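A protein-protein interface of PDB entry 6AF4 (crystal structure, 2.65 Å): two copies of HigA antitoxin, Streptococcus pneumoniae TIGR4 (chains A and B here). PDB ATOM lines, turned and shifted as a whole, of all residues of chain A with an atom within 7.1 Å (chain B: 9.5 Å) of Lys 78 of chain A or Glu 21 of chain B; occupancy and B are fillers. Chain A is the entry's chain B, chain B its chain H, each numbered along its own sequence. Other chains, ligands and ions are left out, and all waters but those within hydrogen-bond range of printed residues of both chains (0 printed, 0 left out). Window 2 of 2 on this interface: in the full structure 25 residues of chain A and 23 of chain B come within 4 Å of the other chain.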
ATOM      1  N   LEU A  50     -33.858 -15.381  12.285  1.00  0.00           N
ATOM      2  CA  LEU A  50     -32.900 -14.598  13.046  1.00  0.00           C
ATOM      3  C   LEU A  50     -32.257 -13.521  12.179  1.00  0.00           C
ATOM      4  O   LEU A  50     -31.939 -12.434  12.660  1.00  0.00           O
ATOM      5  CB  LEU A  50     -31.825 -15.512  13.630  1.00  0.00           C
ATOM      6  CG  LEU A  50     -30.979 -14.954  14.769  1.00  0.00           C
ATOM      7  CD1 LEU A  50     -31.856 -14.396  15.876  1.00  0.00           C
ATOM      8  CD2 LEU A  50     -30.093 -16.048  15.302  1.00  0.00           C
ATOM      9  N   MET A  53     -34.716 -10.476  12.124  1.00  0.00           N
ATOM     10  CA  MET A  53     -34.773  -9.767  13.397  1.00  0.00           C
ATOM     11  C   MET A  53     -33.486  -8.998  13.677  1.00  0.00           C
ATOM     12  O   MET A  53     -33.523  -7.833  14.072  1.00  0.00           O
ATOM     13  CB  MET A  53     -35.043 -10.738  14.543  1.00  0.00           C
ATOM     14  CG  MET A  53     -36.473 -11.211  14.640  1.00  0.00           C
ATOM     15  SD  MET A  53     -36.684 -12.324  16.039  1.00  0.00           S
ATOM     16  CE  MET A  53     -35.375 -13.497  15.720  1.00  0.00           C
ATOM     17  N   SER A  54     -32.352  -9.661  13.486  1.00  0.00           N
ATOM     18  CA  SER A  54     -31.058  -9.082  13.833  1.00  0.00           C
ATOM     19  C   SER A  54     -30.441  -8.226  12.728  1.00  0.00           C
ATOM     20  O   SER A  54     -29.545  -7.422  12.989  1.00  0.00           O
ATOM     21  CB  SER A  54     -30.084 -10.198  14.217  1.00  0.00           C
ATOM     22  OG  SER A  54     -29.903 -11.102  13.140  1.00  0.00           O
ATOM     23  N   GLY A  55     -30.924  -8.387  11.501  1.00  0.00           N
ATOM     24  CA  GLY A  55     -30.384  -7.643  10.375  1.00  0.00           C
ATOM     25  C   GLY A  55     -28.970  -8.027   9.968  1.00  0.00           C
ATOM     26  O   GLY A  55     -28.298  -7.271   9.265  1.00  0.00           O
ATOM     27  N   VAL A  56     -28.508  -9.196  10.407  1.00  0.00           N
ATOM     28  CA  VAL A  56     -27.206  -9.705   9.974  1.00  0.00           C
ATOM     29  C   VAL A  56     -27.399 -10.898   9.042  1.00  0.00           C
ATOM     30  O   VAL A  56     -28.328 -11.685   9.216  1.00  0.00           O
ATOM     31  CB  VAL A  56     -26.312 -10.110  11.167  1.00  0.00           C
ATOM     32  CG1 VAL A  56     -26.027  -8.908  12.051  1.00  0.00           C
ATOM     33  CG2 VAL A  56     -26.965 -11.208  11.973  1.00  0.00           C
ATOM     34  N   MET A  64     -20.609 -17.856  13.091  1.00  0.00           N
ATOM     35  CA  MET A  64     -20.476 -17.791  14.540  1.00  0.00           C
ATOM     36  C   MET A  64     -20.315 -19.207  15.070  1.00  0.00           C
ATOM     37  O   MET A  64     -19.473 -19.472  15.928  1.00  0.00           O
ATOM     38  CB  MET A  64     -21.686 -17.122  15.186  1.00  0.00           C
ATOM     39  CG  MET A  64     -21.754 -15.624  14.992  1.00  0.00           C
ATOM     40  SD  MET A  64     -23.140 -14.927  15.902  1.00  0.00           S
ATOM     41  CE  MET A  64     -22.878 -13.184  15.614  1.00  0.00           C
ATOM     42  N   LEU A  73     -17.492  -8.236  17.097  1.00  0.00           N
ATOM     43  CA  LEU A  73     -18.197  -7.837  18.312  1.00  0.00           C
ATOM     44  C   LEU A  73     -19.572  -7.236  18.042  1.00  0.00           C
ATOM     45  O   LEU A  73     -20.549  -7.597  18.700  1.00  0.00           O
ATOM     46  CB  LEU A  73     -17.353  -6.843  19.114  1.00  0.00           C
ATOM     47  CG  LEU A  73     -17.896  -6.462  20.492  1.00  0.00           C
ATOM     48  CD1 LEU A  73     -18.342  -7.694  21.265  1.00  0.00           C
ATOM     49  CD2 LEU A  73     -16.847  -5.696  21.277  1.00  0.00           C
ATOM     50  N   ASP A  74     -19.646  -6.316  17.085  1.00  0.00           N
ATOM     51  CA  ASP A  74     -20.912  -5.674  16.745  1.00  0.00           C
ATOM     52  C   ASP A  74     -21.916  -6.700  16.226  1.00  0.00           C
ATOM     53  O   ASP A  74     -23.112  -6.608  16.508  1.00  0.00           O
ATOM     54  CB  ASP A  74     -20.699  -4.568  15.707  1.00  0.00           C
ATOM     55  CG  ASP A  74     -20.109  -5.091  14.410  1.00  0.00           C
ATOM     56  OD1 ASP A  74     -19.469  -6.165  14.434  1.00  0.00           O
ATOM     57  OD2 ASP A  74     -20.282  -4.426  13.365  1.00  0.00           O
ATOM     58  N   THR A  75     -21.416  -7.677  15.476  1.00  0.00           N
ATOM     59  CA  THR A  75     -22.254  -8.734  14.925  1.00  0.00           C
ATOM     60  C   THR A  75     -22.872  -9.572  16.036  1.00  0.00           C
ATOM     61  O   THR A  75     -24.050  -9.920  15.984  1.00  0.00           O
ATOM     62  CB  THR A  75     -21.459  -9.655  13.988  1.00  0.00           C
ATOM     63  OG1 THR A  75     -20.761  -8.867  13.017  1.00  0.00           O
ATOM     64  CG2 THR A  75     -22.394 -10.600  13.273  1.00  0.00           C
ATOM     65  N   VAL A  76     -22.065  -9.895  17.041  1.00  0.00           N
ATOM     66  CA  VAL A  76     -22.538 -10.655  18.188  1.00  0.00           C
ATOM     67  C   VAL A  76     -23.602  -9.869  18.953  1.00  0.00           C
ATOM     68  O   VAL A  76     -24.594 -10.436  19.412  1.00  0.00           O
ATOM     69  CB  VAL A  76     -21.379 -11.023  19.136  1.00  0.00           C
ATOM     70  CG1 VAL A  76     -21.905 -11.699  20.386  1.00  0.00           C
ATOM     71  CG2 VAL A  76     -20.381 -11.924  18.428  1.00  0.00           C
ATOM     72  N   LEU A  77     -23.401  -8.561  19.072  1.00  0.00           N
ATOM     73  CA  LEU A  77     -24.328  -7.714  19.815  1.00  0.00           C
ATOM     74  C   LEU A  77     -25.690  -7.600  19.130  1.00  0.00           C
ATOM     75  O   LEU A  77     -26.718  -7.553  19.802  1.00  0.00           O
ATOM     76  CB  LEU A  77     -23.728  -6.325  20.027  1.00  0.00           C
ATOM     77  CG  LEU A  77     -22.571  -6.271  21.029  1.00  0.00           C
ATOM     78  CD1 LEU A  77     -21.981  -4.872  21.094  1.00  0.00           C
ATOM     79  CD2 LEU A  77     -23.022  -6.737  22.410  1.00  0.00           C
ATOM     80  N   LYS A  78     -25.699  -7.557  17.800  1.00  0.00           N
ATOM     81  CA  LYS A  78     -26.953  -7.519  17.053  1.00  0.00           C
ATOM     82  C   LYS A  78     -27.749  -8.802  17.247  1.00  0.00           C
ATOM     83  O   LYS A  78     -28.945  -8.761  17.541  1.00  0.00           O
ATOM     84  CB  LYS A  78     -26.699  -7.299  15.561  1.00  0.00           C
ATOM     85  CG  LYS A  78     -26.152  -5.931  15.208  1.00  0.00           C
ATOM     86  CD  LYS A  78     -26.271  -5.667  13.717  1.00  0.00           C
ATOM     87  CE  LYS A  78     -25.523  -4.410  13.307  1.00  0.00           C
ATOM     88  NZ  LYS A  78     -24.045  -4.596  13.367  1.00  0.00           N
ATOM     89  N   VAL A  79     -27.077  -9.938  17.081  1.00  0.00           N
ATOM     90  CA  VAL A  79     -27.723 -11.240  17.199  1.00  0.00           C
ATOM     91  C   VAL A  79     -28.232 -11.485  18.619  1.00  0.00           C
ATOM     92  O   VAL A  79     -29.364 -11.932  18.810  1.00  0.00           O
ATOM     93  CB  VAL A  79     -26.767 -12.382  16.790  1.00  0.00           C
ATOM     94  CG1 VAL A  79     -27.395 -13.740  17.066  1.00  0.00           C
ATOM     95  CG2 VAL A  79     -26.404 -12.260  15.325  1.00  0.00           C
ATOM     96  N   LEU A  80     -27.403 -11.180  19.613  1.00  0.00           N
ATOM     97  CA  LEU A  80     -27.792 -11.374  21.006  1.00  0.00           C
ATOM     98  C   LEU A  80     -28.976 -10.484  21.387  1.00  0.00           C
ATOM     99  O   LEU A  80     -29.876 -10.917  22.109  1.00  0.00           O
ATOM    100  CB  LEU A  80     -26.611 -11.103  21.943  1.00  0.00           C
ATOM    101  CG  LEU A  80     -25.503 -12.160  22.027  1.00  0.00           C
ATOM    102  CD1 LEU A  80     -24.435 -11.733  23.021  1.00  0.00           C
ATOM    103  CD2 LEU A  80     -26.067 -13.522  22.404  1.00  0.00           C
ATOM    104  N   ALA A  81     -28.975  -9.247  20.899  1.00  0.00           N
ATOM    105  CA  ALA A  81     -30.030  -8.291  21.230  1.00  0.00           C
ATOM    106  C   ALA A  81     -31.391  -8.775  20.750  1.00  0.00           C
ATOM    107  O   ALA A  81     -32.389  -8.646  21.460  1.00  0.00           O
ATOM    108  CB  ALA A  81     -29.718  -6.922  20.640  1.00  0.00           C
ATOM    109  N   SER A  82     -31.431  -9.341  19.548  1.00  0.00           N
ATOM    110  CA  SER A  82     -32.682  -9.846  18.997  1.00  0.00           C
ATOM    111  C   SER A  82     -33.182 -11.043  19.804  1.00  0.00           C
ATOM    112  O   SER A  82     -34.359 -11.394  19.745  1.00  0.00           O
ATOM    113  CB  SER A  82     -32.511 -10.225  17.526  1.00  0.00           C
ATOM    114  OG  SER A  82     -31.815 -11.449  17.390  1.00  0.00           O
ATOM    115  N   LEU A  83     -32.281 -11.665  20.558  1.00  0.00           N
ATOM    116  CA  LEU A  83     -32.637 -12.789  21.420  1.00  0.00           C
ATOM    117  C   LEU A  83     -32.891 -12.349  22.860  1.00  0.00           C
ATOM    118  O   LEU A  83     -33.137 -13.181  23.734  1.00  0.00           O
ATOM    119  CB  LEU A  83     -31.541 -13.856  21.384  1.00  0.00           C
ATOM    120  CG  LEU A  83     -31.362 -14.556  20.034  1.00  0.00           C
ATOM    121  CD1 LEU A  83     -30.261 -15.602  20.107  1.00  0.00           C
ATOM    122  CD2 LEU A  83     -32.671 -15.183  19.577  1.00  0.00           C
ATOM    123  N   LYS A  85     -30.651 -10.584  24.724  1.00  0.00           N
ATOM    124  CA  LYS A  85     -29.401 -10.695  25.465  1.00  0.00           C
ATOM    125  C   LYS A  85     -28.396  -9.644  25.013  1.00  0.00           C
ATOM    126  O   LYS A  85     -28.570  -9.013  23.974  1.00  0.00           O
ATOM    127  CB  LYS A  85     -28.802 -12.092  25.293  1.00  0.00           C
ATOM    128  CG  LYS A  85     -29.636 -13.216  25.888  1.00  0.00           C
ATOM    129  CD  LYS A  85     -29.460 -13.295  27.398  1.00  0.00           C
ATOM    130  CE  LYS A  85     -30.434 -14.286  28.018  1.00  0.00           C
ATOM    131  NZ  LYS A  85     -30.357 -15.624  27.368  1.00  0.00           N
ATOM    132  N   ARG B  14     -29.864  11.788  22.918  1.00  0.00           N
ATOM    133  CA  ARG B  14     -29.317  10.507  22.476  1.00  0.00           C
ATOM    134  C   ARG B  14     -30.417   9.480  22.202  1.00  0.00           C
ATOM    135  O   ARG B  14     -30.372   8.752  21.208  1.00  0.00           O
ATOM    136  CB  ARG B  14     -28.346   9.958  23.525  1.00  0.00           C
ATOM    137  CG  ARG B  14     -27.594   8.717  23.091  1.00  0.00           C
ATOM    138  CD  ARG B  14     -26.708   8.185  24.208  1.00  0.00           C
ATOM    139  NE  ARG B  14     -25.654   7.321  23.686  1.00  0.00           N
ATOM    140  CZ  ARG B  14     -25.135   6.289  24.343  1.00  0.00           C
ATOM    141  NH1 ARG B  14     -25.578   5.980  25.554  1.00  0.00           N
ATOM    142  NH2 ARG B  14     -24.178   5.562  23.783  1.00  0.00           N
ATOM    143  N   ALA B  15     -31.401   9.427  23.092  1.00  0.00           N
ATOM    144  CA  ALA B  15     -32.499   8.478  22.970  1.00  0.00           C
ATOM    145  C   ALA B  15     -33.351   8.759  21.734  1.00  0.00           C
ATOM    146  O   ALA B  15     -33.909   7.840  21.137  1.00  0.00           O
ATOM    147  CB  ALA B  15     -33.360   8.504  24.226  1.00  0.00           C
ATOM    148  N   PHE B  18     -31.019   8.090  18.140  1.00  0.00           N
ATOM    149  CA  PHE B  18     -30.407   6.779  17.930  1.00  0.00           C
ATOM    150  C   PHE B  18     -31.336   5.637  18.319  1.00  0.00           C
ATOM    151  O   PHE B  18     -32.095   5.740  19.284  1.00  0.00           O
ATOM    152  CB  PHE B  18     -29.098   6.668  18.719  1.00  0.00           C
ATOM    153  CG  PHE B  18     -28.060   7.675  18.316  1.00  0.00           C
ATOM    154  CD1 PHE B  18     -27.213   7.426  17.249  1.00  0.00           C
ATOM    155  CD2 PHE B  18     -27.928   8.868  19.005  1.00  0.00           C
ATOM    156  CE1 PHE B  18     -26.262   8.350  16.872  1.00  0.00           C
ATOM    157  CE2 PHE B  18     -26.975   9.797  18.635  1.00  0.00           C
ATOM    158  CZ  PHE B  18     -26.140   9.538  17.567  1.00  0.00           C
ATOM    159  N   SER B  19     -31.267   4.548  17.561  1.00  0.00           N
ATOM    160  CA  SER B  19     -32.044   3.354  17.870  1.00  0.00           C
ATOM    161  C   SER B  19     -31.463   2.661  19.094  1.00  0.00           C
ATOM    162  O   SER B  19     -30.308   2.896  19.451  1.00  0.00           O
ATOM    163  CB  SER B  19     -32.071   2.398  16.675  1.00  0.00           C
ATOM    164  OG  SER B  19     -30.769   1.939  16.351  1.00  0.00           O
ATOM    165  N   LYS B  20     -32.271   1.825  19.742  1.00  0.00           N
ATOM    166  CA  LYS B  20     -31.821   1.043  20.894  1.00  0.00           C
ATOM    167  C   LYS B  20     -30.564   0.246  20.549  1.00  0.00           C
ATOM    168  O   LYS B  20     -29.647   0.124  21.361  1.00  0.00           O
ATOM    169  CB  LYS B  20     -32.922   0.095  21.369  1.00  0.00           C
ATOM    170  CG  LYS B  20     -34.107   0.780  22.043  1.00  0.00           C
ATOM    171  CD  LYS B  20     -35.183  -0.241  22.411  1.00  0.00           C
ATOM    172  CE  LYS B  20     -36.245   0.352  23.332  1.00  0.00           C
ATOM    173  NZ  LYS B  20     -37.107   1.357  22.644  1.00  0.00           N
ATOM    174  N   GLU B  21     -30.536  -0.282  19.331  1.00  0.00           N
ATOM    175  CA  GLU B  21     -29.401  -1.030  18.801  1.00  0.00           C
ATOM    176  C   GLU B  21     -28.125  -0.200  18.707  1.00  0.00           C
ATOM    177  O   GLU B  21     -27.055  -0.639  19.118  1.00  0.00           O
ATOM    178  CB  GLU B  21     -29.765  -1.577  17.420  1.00  0.00           C
ATOM    179  CG  GLU B  21     -28.581  -1.978  16.557  1.00  0.00           C
ATOM    180  CD  GLU B  21     -28.931  -1.945  15.082  1.00  0.00           C
ATOM    181  OE1 GLU B  21     -30.017  -1.423  14.746  1.00  0.00           O
ATOM    182  OE2 GLU B  21     -28.124  -2.429  14.263  1.00  0.00           O
ATOM    183  N   GLU B  22     -28.249   0.999  18.150  1.00  0.00           N
ATOM    184  CA  GLU B  22     -27.102   1.877  17.946  1.00  0.00           C
ATOM    185  C   GLU B  22     -26.503   2.320  19.268  1.00  0.00           C
ATOM    186  O   GLU B  22     -25.291   2.483  19.388  1.00  0.00           O
ATOM    187  CB  GLU B  22     -27.507   3.102  17.128  1.00  0.00           C
ATOM    188  CG  GLU B  22     -27.702   2.813  15.657  1.00  0.00           C
ATOM    189  CD  GLU B  22     -28.378   3.953  14.927  1.00  0.00           C
ATOM    190  OE1 GLU B  22     -29.255   4.615  15.528  1.00  0.00           O
ATOM    191  OE2 GLU B  22     -28.030   4.190  13.751  1.00  0.00           O
ATOM    192  N   ILE B  23     -27.366   2.504  20.261  1.00  0.00           N
ATOM    193  CA  ILE B  23     -26.939   2.946  21.580  1.00  0.00           C
ATOM    194  C   ILE B  23     -26.164   1.849  22.305  1.00  0.00           C
ATOM    195  O   ILE B  23     -25.125   2.113  22.907  1.00  0.00           O
ATOM    196  CB  ILE B  23     -28.145   3.394  22.431  1.00  0.00           C
ATOM    197  CG1 ILE B  23     -28.681   4.729  21.911  1.00  0.00           C
ATOM    198  CG2 ILE B  23     -27.764   3.523  23.901  1.00  0.00           C
ATOM    199  CD1 ILE B  23     -29.931   5.204  22.618  1.00  0.00           C
ATOM    200  N   LEU B  24     -26.657   0.617  22.228  1.00  0.00           N
ATOM    201  CA  LEU B  24     -25.994  -0.500  22.893  1.00  0.00           C
ATOM    202  C   LEU B  24     -24.597  -0.720  22.305  1.00  0.00           C
ATOM    203  O   LEU B  24     -23.626  -0.904  23.043  1.00  0.00           O
ATOM    204  CB  LEU B  24     -26.838  -1.769  22.770  1.00  0.00           C
ATOM    205  CG  LEU B  24     -26.799  -2.811  23.896  1.00  0.00           C
ATOM    206  CD1 LEU B  24     -27.687  -3.976  23.507  1.00  0.00           C
ATOM    207  CD2 LEU B  24     -25.387  -3.293  24.238  1.00  0.00           C
ATOM    208  N   GLU B  25     -24.493  -0.691  20.981  1.00  0.00           N
ATOM    209  CA  GLU B  25     -23.197  -0.860  20.332  1.00  0.00           C
ATOM    210  C   GLU B  25     -22.281   0.322  20.616  1.00  0.00           C
ATOM    211  O   GLU B  25     -21.062   0.171  20.686  1.00  0.00           O
ATOM    212  CB  GLU B  25     -23.365  -1.043  18.829  1.00  0.00           C
ATOM    213  CG  GLU B  25     -23.999  -2.359  18.457  1.00  0.00           C
ATOM    214  CD  GLU B  25     -24.038  -2.574  16.968  1.00  0.00           C
ATOM    215  OE1 GLU B  25     -23.219  -1.956  16.255  1.00  0.00           O
ATOM    216  OE2 GLU B  25     -24.891  -3.359  16.510  1.00  0.00           O
ATOM    217  N   SER B  26     -22.873   1.500  20.782  1.00  0.00           N
ATOM    218  CA  SER B  26     -22.110   2.680  21.158  1.00  0.00           C
ATOM    219  C   SER B  26     -21.590   2.534  22.581  1.00  0.00           C
ATOM    220  O   SER B  26     -20.445   2.884  22.868  1.00  0.00           O
ATOM    221  CB  SER B  26     -22.963   3.942  21.031  1.00  0.00           C
ATOM    222  OG  SER B  26     -22.250   5.082  21.475  1.00  0.00           O
ATOM    223  N   ASP B  27     -22.434   2.006  23.467  1.00  0.00           N
ATOM    224  CA  ASP B  27     -22.057   1.803  24.864  1.00  0.00           C
ATOM    225  C   ASP B  27     -20.911   0.802  25.000  1.00  0.00           C
ATOM    226  O   ASP B  27     -20.077   0.921  25.896  1.00  0.00           O
ATOM    227  CB  ASP B  27     -23.257   1.331  25.690  1.00  0.00           C
ATOM    228  CG  ASP B  27     -24.174   2.472  26.098  1.00  0.00           C
ATOM    229  OD1 ASP B  27     -23.736   3.641  26.049  1.00  0.00           O
ATOM    230  OD2 ASP B  27     -25.333   2.198  26.478  1.00  0.00           O
ATOM    231  N   MET B  28     -20.872  -0.180  24.107  1.00  0.00           N
ATOM    232  CA  MET B  28     -19.804  -1.170  24.126  1.00  0.00           C
ATOM    233  C   MET B  28     -18.491  -0.554  23.659  1.00  0.00           C
ATOM    234  O   MET B  28     -17.436  -0.821  24.232  1.00  0.00           O
ATOM    235  CB  MET B  28     -20.163  -2.376  23.254  1.00  0.00           C
ATOM    236  CG  MET B  28     -19.081  -3.448  23.217  1.00  0.00           C
ATOM    237  SD  MET B  28     -18.598  -4.012  24.865  1.00  0.00           S
ATOM    238  CE  MET B  28     -20.072  -4.887  25.381  1.00  0.00           C
ATOM    239  N   ARG B  29     -18.559   0.274  22.620  1.00  0.00           N
ATOM    240  CA  ARG B  29     -17.366   0.933  22.099  1.00  0.00           C
ATOM    241  C   ARG B  29     -16.756   1.880  23.129  1.00  0.00           C
ATOM    242  O   ARG B  29     -15.537   1.947  23.263  1.00  0.00           O
ATOM    243  CB  ARG B  29     -17.681   1.698  20.810  1.00  0.00           C
ATOM    244  CG  ARG B  29     -17.918   0.808  19.598  1.00  0.00           C
ATOM    245  CD  ARG B  29     -17.815   1.595  18.297  1.00  0.00           C
ATOM    246  NE  ARG B  29     -18.793   2.678  18.222  1.00  0.00           N
ATOM    247  CZ  ARG B  29     -20.053   2.524  17.821  1.00  0.00           C
ATOM    248  NH1 ARG B  29     -20.498   1.329  17.460  1.00  0.00           N
ATOM    249  NH2 ARG B  29     -20.871   3.567  17.784  1.00  0.00           N
ATOM    250  N   SER B  70     -15.131  -3.235  13.820  1.00  0.00           N
ATOM    251  CA  SER B  70     -15.379  -3.930  15.076  1.00  0.00           C
ATOM    252  C   SER B  70     -14.377  -5.067  15.278  1.00  0.00           C
ATOM    253  O   SER B  70     -14.121  -5.846  14.361  1.00  0.00           O
ATOM    254  CB  SER B  70     -16.815  -4.462  15.113  1.00  0.00           C
ATOM    255  OG  SER B  70     -17.128  -5.030  16.373  1.00  0.00           O
ATOM    256  N   LEU B  92     -30.880  -8.351  28.399  1.00  0.00           N
ATOM    257  CA  LEU B  92     -31.144  -7.005  27.915  1.00  0.00           C
ATOM    258  C   LEU B  92     -32.106  -6.293  28.865  1.00  0.00           C
ATOM    259  O   LEU B  92     -32.946  -6.936  29.494  1.00  0.00           O
ATOM    260  CB  LEU B  92     -31.724  -7.060  26.500  1.00  0.00           C
ATOM    261  CG  LEU B  92     -31.630  -5.794  25.655  1.00  0.00           C
ATOM    262  CD1 LEU B  92     -30.184  -5.344  25.584  1.00  0.00           C
ATOM    263  CD2 LEU B  92     -32.188  -6.053  24.262  1.00  0.00           C
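The backbone NH (N) of Asp 74 of chain A sits at hydrogen-bond distance from the side-chain hydroxyl (OG) of Ser 70 of chain B (2.9 Å).
NZ of Lys 78 of chain A lies within salt-bridge range of OE2 of Glu 25 of chain B (3.5 Å).
The side-chain hydroxyl (OG) of Ser 70 of chain B sits close to the backbone NH (N) of Leu 73 of chain A, 3.3 Å away.
The backbone carbonyl oxygen (O) of Glu 25 of chain B sits close to the guanidinium group (NH1) of Arg 29 of chain B (3.5 Å).
The side-chain amino group (NZ) of Lys 78 of chain A lies within salt-bridge range of the side-chain carboxylate (OD2) of Asp 74 of chain A (3.8 Å).
The side-chain carboxylate of Asp 74 of chain A lies within hydrogen-bond range of the side-chain hydroxyl of Thr 75 of chain A, 3.3 Å away.
No residue of chain B comes within 4 Å of Ser 54 of chain A.
Val 56 of chain A touches none of the printed residues of chain B.
Of the printed residues of chain B, Leu 73 of chain A touches Met 28 and Ser 70.
Of chain B, only Glu 21 (3.4 Å) and Glu 25 (3.1 Å) come within 4 Å of Lys 78 of chain A.
Ala 81 of chain A touches one residue of chain B.
Of chain A, only Lys 78 comes within 4 Å of Glu 21 of chain B.
Of the printed residues of chain A, Glu 25 of chain B touches Asp 74 (3.7 Å) and Lys 78 (3.1 Å).
Hydrophobic or aromatic side chains of chain B that line the printed part of chain A: Met 28 and Leu 92.
Of the 18 printed residues of chain A, 5 touch a printed residue of chain B.
Among the printed residues, 8 pairs touch across the chains.
Among the printed residues, pairs that only touch across the chains: Leu 73 of chain A with Met 28 of chain B, Asp 74 of chain A with Glu 25 of chain B, Leu 77 of chain A with Met 28 of chain B, Lys 78 of chain A with Glu 21 of chain B and Ala 81 of chain A with Leu 92 of chain B.
No position is printed for both chains.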
